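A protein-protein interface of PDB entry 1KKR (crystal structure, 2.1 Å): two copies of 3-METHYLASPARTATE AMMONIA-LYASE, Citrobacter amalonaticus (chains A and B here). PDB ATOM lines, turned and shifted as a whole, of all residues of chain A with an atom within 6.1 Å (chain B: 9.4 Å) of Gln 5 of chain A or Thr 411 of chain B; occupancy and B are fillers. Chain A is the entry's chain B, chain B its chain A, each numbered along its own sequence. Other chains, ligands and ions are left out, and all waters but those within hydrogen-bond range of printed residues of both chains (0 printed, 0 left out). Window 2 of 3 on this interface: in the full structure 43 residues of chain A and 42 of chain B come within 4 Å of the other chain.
The side-chain amide nitrogen (NE2) of Gln 56 of chain A is in hydrogen-bond range of the backbone carbonyl oxygen (O) of Arg 404 of chain B (3.1 Å).
The side-chain amide oxygen (OE1) of Gln 5 of chain A sits at hydrogen-bond distance from the side-chain amino group (NZ) of Lys 4 of chain A.
N of Lys 4 of chain A sits at hydrogen-bond distance from O of Ile 58 of chain A.
O of Gln 5 of chain A is in hydrogen-bond range of N of Ile 58 of chain A.
N of Leu 7 of chain A lies within hydrogen-bond range of O of Gln 56 of chain A, 2.8 Å away.
Gln 5 of chain A touches Thr 411 of chain B.
Leu 7 of chain A touches Ala 407 of chain B (CD1 to O, 3.9 Å).
CD1 of Leu 7 of chain A touches CD2 of Leu 408 of chain B (3.9 Å).
Gln 56 of chain A touches Leu 408 of chain B.
Leu 408 of chain B touches Ile 58 of chain A.
Of chain A, only Gln 5 (3.6 Å) comes within 4 Å of Thr 411 of chain B.
No residue of chain B comes within 4 Å of Lys 4 of chain A.
No residue of chain B comes within 4 Å of Ala 6 of chain A.
Of chain B, only Leu 408 comes within 4 Å of Ile 58 of chain A.
Of the printed residues of chain B, Leu 7 of chain A touches Ala 407 and Leu 408.
Printed residues of chain A within 4 Å of Leu 408 of chain B: Leu 7, Gln 56 and Ile 58.
Of the printed residues of chain B, Gln 56 of chain A touches Arg 404 and Leu 408.
Leu 59 of chain A touches none of the printed residues of chain B.
The nearest residue of chain B that does not touch Gln 5 of chain A is Ala 407 of chain B (6.9 Å).
The nearest residue of chain A that does not touch Thr 411 of chain B is Leu 7 of chain A (4.1 Å).
Printed residues of chain B that touch a printed residue of chain A: Arg 404, Ala 407, Leu 408 and Thr 411.
Of the 11 printed residues of chain A, 4 touch a printed residue of chain B.
Hydrophobic or aromatic side chains of chain A within 4 Å of the printed part of chain B: Leu 7 and Ile 58.
Among the printed residues, no Asp or Glu carboxylate lies within 4 Å of a Lys or Arg side-chain nitrogen of the other chain.
No position is printed for both chains.
Of the 6 pairs that touch across the chains among the printed residues, none has its exchanged pair printed and touching as well.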
ATOM      1  N   ILE A   3      -1.339   5.530 -24.517  1.00  0.00           N
ATOM      2  CA  ILE A   3      -2.672   4.993 -24.644  1.00  0.00           C
ATOM      3  C   ILE A   3      -3.161   5.759 -25.859  1.00  0.00           C
ATOM      4  O   ILE A   3      -2.929   6.972 -25.946  1.00  0.00           O
ATOM      5  CB  ILE A   3      -3.524   5.412 -23.442  1.00  0.00           C
ATOM      6  CG1 ILE A   3      -3.056   4.749 -22.154  1.00  0.00           C
ATOM      7  CG2 ILE A   3      -4.992   5.201 -23.728  1.00  0.00           C
ATOM      8  CD1 ILE A   3      -3.654   5.433 -20.922  1.00  0.00           C
ATOM      9  N   LYS A   4      -3.845   5.051 -26.746  1.00  0.00           N
ATOM     10  CA  LYS A   4      -4.329   5.573 -27.994  1.00  0.00           C
ATOM     11  C   LYS A   4      -5.783   5.826 -27.812  1.00  0.00           C
ATOM     12  O   LYS A   4      -6.269   6.824 -28.241  1.00  0.00           O
ATOM     13  CB  LYS A   4      -4.083   4.577 -29.152  1.00  0.00           C
ATOM     14  CG  LYS A   4      -4.898   4.899 -30.377  1.00  0.00           C
ATOM     15  CD  LYS A   4      -4.693   3.858 -31.481  1.00  0.00           C
ATOM     16  CE  LYS A   4      -5.872   2.800 -31.513  1.00  0.00           C
ATOM     17  NZ  LYS A   4      -7.260   3.316 -31.112  1.00  0.00           N
ATOM     18  N   GLN A   5      -6.487   4.938 -27.137  1.00  0.00           N
ATOM     19  CA  GLN A   5      -7.890   5.141 -26.948  1.00  0.00           C
ATOM     20  C   GLN A   5      -8.396   4.551 -25.629  1.00  0.00           C
ATOM     21  O   GLN A   5      -7.912   3.509 -25.202  1.00  0.00           O
ATOM     22  CB  GLN A   5      -8.531   4.449 -28.109  1.00  0.00           C
ATOM     23  CG  GLN A   5      -9.851   4.951 -28.371  1.00  0.00           C
ATOM     24  CD  GLN A   5     -10.431   4.408 -29.652  1.00  0.00           C
ATOM     25  OE1 GLN A   5      -9.744   3.750 -30.430  1.00  0.00           O
ATOM     26  NE2 GLN A   5     -11.702   4.685 -29.874  1.00  0.00           N
ATOM     27  N   ALA A   6      -9.352   5.207 -24.981  1.00  0.00           N
ATOM     28  CA  ALA A   6      -9.905   4.682 -23.727  1.00  0.00           C
ATOM     29  C   ALA A   6     -11.401   4.458 -23.901  1.00  0.00           C
ATOM     30  O   ALA A   6     -12.105   5.347 -24.362  1.00  0.00           O
ATOM     31  CB  ALA A   6      -9.603   5.613 -22.592  1.00  0.00           C
ATOM     32  N   LEU A   7     -11.881   3.252 -23.605  1.00  0.00           N
ATOM     33  CA  LEU A   7     -13.296   2.938 -23.753  1.00  0.00           C
ATOM     34  C   LEU A   7     -13.827   2.590 -22.388  1.00  0.00           C
ATOM     35  O   LEU A   7     -13.131   1.987 -21.584  1.00  0.00           O
ATOM     36  CB  LEU A   7     -13.500   1.732 -24.632  1.00  0.00           C
ATOM     37  CG  LEU A   7     -12.791   1.707 -25.981  1.00  0.00           C
ATOM     38  CD1 LEU A   7     -13.250   0.511 -26.770  1.00  0.00           C
ATOM     39  CD2 LEU A   7     -13.068   2.948 -26.786  1.00  0.00           C
ATOM     40  N   GLN A  56     -11.099   0.096 -20.757  1.00  0.00           N
ATOM     41  CA  GLN A  56     -10.170  -0.560 -21.700  1.00  0.00           C
ATOM     42  C   GLN A  56      -9.300   0.492 -22.332  1.00  0.00           C
ATOM     43  O   GLN A  56      -9.833   1.471 -22.935  1.00  0.00           O
ATOM     44  CB  GLN A  56     -10.915  -1.266 -22.810  1.00  0.00           C
ATOM     45  CG  GLN A  56     -11.775  -2.516 -22.367  1.00  0.00           C
ATOM     46  CD  GLN A  56     -12.441  -3.229 -23.525  1.00  0.00           C
ATOM     47  OE1 GLN A  56     -11.974  -4.301 -23.954  1.00  0.00           O
ATOM     48  NE2 GLN A  56     -13.573  -2.675 -23.998  1.00  0.00           N
ATOM     49  N   LEU A  57      -7.986   0.246 -22.290  1.00  0.00           N
ATOM     50  CA  LEU A  57      -7.004   1.188 -22.826  1.00  0.00           C
ATOM     51  C   LEU A  57      -6.278   0.552 -23.993  1.00  0.00           C
ATOM     52  O   LEU A  57      -5.430  -0.345 -23.836  1.00  0.00           O
ATOM     53  CB  LEU A  57      -6.013   1.665 -21.772  1.00  0.00           C
ATOM     54  CG  LEU A  57      -6.622   2.150 -20.477  1.00  0.00           C
ATOM     55  CD1 LEU A  57      -5.543   2.338 -19.428  1.00  0.00           C
ATOM     56  CD2 LEU A  57      -7.501   3.375 -20.632  1.00  0.00           C
ATOM     57  N   ILE A  58      -6.623   0.980 -25.192  1.00  0.00           N
ATOM     58  CA  ILE A  58      -5.898   0.465 -26.353  1.00  0.00           C
ATOM     59  C   ILE A  58      -4.596   1.222 -26.484  1.00  0.00           C
ATOM     60  O   ILE A  58      -4.589   2.433 -26.642  1.00  0.00           O
ATOM     61  CB  ILE A  58      -6.708   0.667 -27.598  1.00  0.00           C
ATOM     62  CG1 ILE A  58      -8.088   0.048 -27.408  1.00  0.00           C
ATOM     63  CG2 ILE A  58      -5.939   0.089 -28.808  1.00  0.00           C
ATOM     64  CD1 ILE A  58      -9.001   0.271 -28.570  1.00  0.00           C
ATOM     65  N   LEU A  59      -3.483   0.553 -26.305  1.00  0.00           N
ATOM     66  CA  LEU A  59      -2.196   1.235 -26.464  1.00  0.00           C
ATOM     67  C   LEU A  59      -1.685   1.247 -27.922  1.00  0.00           C
ATOM     68  O   LEU A  59      -2.237   0.564 -28.780  1.00  0.00           O
ATOM     69  CB  LEU A  59      -1.167   0.511 -25.633  1.00  0.00           C
ATOM     70  CG  LEU A  59      -1.658   0.023 -24.277  1.00  0.00           C
ATOM     71  CD1 LEU A  59      -0.538  -0.627 -23.595  1.00  0.00           C
ATOM     72  CD2 LEU A  59      -2.177   1.179 -23.472  1.00  0.00           C
ATOM     73  N   GLU A 102      -6.114   9.605 -23.251  1.00  0.00           N
ATOM     74  CA  GLU A 102      -5.777   9.423 -24.655  1.00  0.00           C
ATOM     75  C   GLU A 102      -4.576  10.291 -24.957  1.00  0.00           C
ATOM     76  O   GLU A 102      -4.582  11.507 -24.760  1.00  0.00           O
ATOM     77  CB  GLU A 102      -6.988   9.717 -25.490  1.00  0.00           C
ATOM     78  CG  GLU A 102      -8.124   8.761 -25.138  1.00  0.00           C
ATOM     79  CD  GLU A 102      -9.215   8.748 -26.188  1.00  0.00           C
ATOM     80  OE1 GLU A 102      -9.967   7.723 -26.306  1.00  0.00           O
ATOM     81  OE2 GLU A 102      -9.302   9.795 -26.884  1.00  0.00           O
ATOM     82  N   GLY A 103      -3.494   9.609 -25.297  1.00  0.00           N
ATOM     83  CA  GLY A 103      -2.211  10.255 -25.442  1.00  0.00           C
ATOM     84  C   GLY A 103      -1.312  10.080 -24.208  1.00  0.00           C
ATOM     85  O   GLY A 103      -0.164  10.465 -24.257  1.00  0.00           O
ATOM     86  N   LEU B 149      -8.444  -9.545 -31.970  1.00  0.00           N
ATOM     87  CA  LEU B 149      -9.190 -10.207 -30.920  1.00  0.00           C
ATOM     88  C   LEU B 149      -9.455 -11.642 -31.363  1.00  0.00           C
ATOM     89  O   LEU B 149      -9.520 -11.919 -32.580  1.00  0.00           O
ATOM     90  CB  LEU B 149     -10.537  -9.530 -30.753  1.00  0.00           C
ATOM     91  CG  LEU B 149     -10.432  -8.011 -30.515  1.00  0.00           C
ATOM     92  CD1 LEU B 149     -11.789  -7.393 -30.195  1.00  0.00           C
ATOM     93  CD2 LEU B 149      -9.517  -7.710 -29.368  1.00  0.00           C
ATOM     94  N   GLU B 152     -12.126 -11.867 -33.991  1.00  0.00           N
ATOM     95  CA  GLU B 152     -11.686 -11.569 -35.354  1.00  0.00           C
ATOM     96  C   GLU B 152     -10.963 -12.731 -36.016  1.00  0.00           C
ATOM     97  O   GLU B 152     -11.103 -12.934 -37.216  1.00  0.00           O
ATOM     98  CB  GLU B 152     -10.836 -10.311 -35.419  1.00  0.00           C
ATOM     99  CG  GLU B 152     -11.574  -9.094 -34.918  1.00  0.00           C
ATOM    100  CD  GLU B 152     -10.669  -7.889 -34.735  1.00  0.00           C
ATOM    101  OE1 GLU B 152      -9.614  -7.945 -34.067  1.00  0.00           O
ATOM    102  OE2 GLU B 152     -11.017  -6.862 -35.291  1.00  0.00           O
ATOM    103  N   PRO B 164     -20.862  -6.765 -35.076  1.00  0.00           N
ATOM    104  CA  PRO B 164     -20.817  -6.793 -33.604  1.00  0.00           C
ATOM    105  C   PRO B 164     -22.195  -6.689 -32.972  1.00  0.00           C
ATOM    106  O   PRO B 164     -22.833  -5.635 -32.947  1.00  0.00           O
ATOM    107  CB  PRO B 164     -19.925  -5.600 -33.258  1.00  0.00           C
ATOM    108  CG  PRO B 164     -19.405  -5.044 -34.608  1.00  0.00           C
ATOM    109  CD  PRO B 164     -20.373  -5.504 -35.625  1.00  0.00           C
ATOM    110  N   ARG B 404     -17.514  -5.714 -23.700  1.00  0.00           N
ATOM    111  CA  ARG B 404     -16.194  -5.113 -23.901  1.00  0.00           C
ATOM    112  C   ARG B 404     -15.770  -5.378 -25.334  1.00  0.00           C
ATOM    113  O   ARG B 404     -15.149  -4.528 -25.986  1.00  0.00           O
ATOM    114  CB  ARG B 404     -15.095  -5.670 -22.974  1.00  0.00           C
ATOM    115  CG  ARG B 404     -15.107  -5.223 -21.534  1.00  0.00           C
ATOM    116  CD  ARG B 404     -13.854  -5.657 -20.785  1.00  0.00           C
ATOM    117  NE  ARG B 404     -13.848  -7.079 -20.532  1.00  0.00           N
ATOM    118  CZ  ARG B 404     -14.455  -7.652 -19.515  1.00  0.00           C
ATOM    119  NH1 ARG B 404     -15.094  -6.912 -18.635  1.00  0.00           N
ATOM    120  NH2 ARG B 404     -14.388  -8.971 -19.350  1.00  0.00           N
ATOM    121  N   THR B 405     -16.155  -6.541 -25.830  1.00  0.00           N
ATOM    122  CA  THR B 405     -15.579  -7.020 -27.061  1.00  0.00           C
ATOM    123  C   THR B 405     -16.286  -6.322 -28.199  1.00  0.00           C
ATOM    124  O   THR B 405     -15.650  -5.962 -29.214  1.00  0.00           O
ATOM    125  CB  THR B 405     -15.673  -8.561 -27.181  1.00  0.00           C
ATOM    126  OG1 THR B 405     -14.886  -9.215 -26.143  1.00  0.00           O
ATOM    127  CG2 THR B 405     -15.132  -9.005 -28.535  1.00  0.00           C
ATOM    128  N   ILE B 406     -17.587  -6.105 -28.010  1.00  0.00           N
ATOM    129  CA  ILE B 406     -18.415  -5.428 -29.000  1.00  0.00           C
ATOM    130  C   ILE B 406     -17.891  -4.005 -29.122  1.00  0.00           C
ATOM    131  O   ILE B 406     -17.649  -3.520 -30.220  1.00  0.00           O
ATOM    132  CB  ILE B 406     -19.941  -5.508 -28.623  1.00  0.00           C
ATOM    133  CG1 ILE B 406     -20.498  -6.899 -28.885  1.00  0.00           C
ATOM    134  CG2 ILE B 406     -20.783  -4.475 -29.395  1.00  0.00           C
ATOM    135  CD1 ILE B 406     -21.959  -7.033 -28.509  1.00  0.00           C
ATOM    136  N   ALA B 407     -17.636  -3.354 -27.987  1.00  0.00           N
ATOM    137  CA  ALA B 407     -17.071  -2.013 -28.042  1.00  0.00           C
ATOM    138  C   ALA B 407     -15.754  -1.977 -28.767  1.00  0.00           C
ATOM    139  O   ALA B 407     -15.530  -1.022 -29.509  1.00  0.00           O
ATOM    140  CB  ALA B 407     -16.924  -1.357 -26.659  1.00  0.00           C
ATOM    141  N   LEU B 408     -14.842  -2.925 -28.495  1.00  0.00           N
ATOM    142  CA  LEU B 408     -13.553  -2.886 -29.142  1.00  0.00           C
ATOM    143  C   LEU B 408     -13.804  -3.015 -30.652  1.00  0.00           C
ATOM    144  O   LEU B 408     -13.214  -2.290 -31.456  1.00  0.00           O
ATOM    145  CB  LEU B 408     -12.582  -3.988 -28.686  1.00  0.00           C
ATOM    146  CG  LEU B 408     -11.886  -3.831 -27.314  1.00  0.00           C
ATOM    147  CD1 LEU B 408     -11.112  -5.118 -26.913  1.00  0.00           C
ATOM    148  CD2 LEU B 408     -10.946  -2.608 -27.409  1.00  0.00           C
ATOM    149  N   LEU B 409     -14.635  -3.972 -31.039  1.00  0.00           N
ATOM    150  CA  LEU B 409     -14.890  -4.176 -32.449  1.00  0.00           C
ATOM    151  C   LEU B 409     -15.463  -2.934 -33.154  1.00  0.00           C
ATOM    152  O   LEU B 409     -15.228  -2.733 -34.317  1.00  0.00           O
ATOM    153  CB  LEU B 409     -15.856  -5.356 -32.646  1.00  0.00           C
ATOM    154  CG  LEU B 409     -15.151  -6.710 -32.452  1.00  0.00           C
ATOM    155  CD1 LEU B 409     -16.200  -7.716 -32.247  1.00  0.00           C
ATOM    156  CD2 LEU B 409     -14.340  -7.149 -33.620  1.00  0.00           C
ATOM    157  N   GLN B 410     -16.239  -2.132 -32.449  1.00  0.00           N
ATOM    158  CA  GLN B 410     -16.969  -1.013 -33.056  1.00  0.00           C
ATOM    159  C   GLN B 410     -16.041   0.159 -33.339  1.00  0.00           C
ATOM    160  O   GLN B 410     -16.372   1.092 -34.061  1.00  0.00           O
ATOM    161  CB  GLN B 410     -18.114  -0.602 -32.142  1.00  0.00           C
ATOM    162  CG  GLN B 410     -19.344  -1.470 -32.338  1.00  0.00           C
ATOM    163  CD  GLN B 410     -20.516  -1.263 -31.343  1.00  0.00           C
ATOM    164  OE1 GLN B 410     -21.619  -1.760 -31.596  1.00  0.00           O
ATOM    165  NE2 GLN B 410     -20.273  -0.601 -30.221  1.00  0.00           N
ATOM    166  N   THR B 411     -14.845   0.041 -32.796  1.00  0.00           N
ATOM    167  CA  THR B 411     -13.776   1.006 -32.891  1.00  0.00           C
ATOM    168  C   THR B 411     -13.135   1.167 -34.285  1.00  0.00           C
ATOM    169  O   THR B 411     -13.048   0.192 -35.052  1.00  0.00           O
ATOM    170  CB  THR B 411     -12.774   0.452 -31.875  1.00  0.00           C
ATOM    171  OG1 THR B 411     -12.668   1.325 -30.742  1.00  0.00           O
ATOM    172  CG2 THR B 411     -11.442   0.294 -32.432  1.00  0.00           C
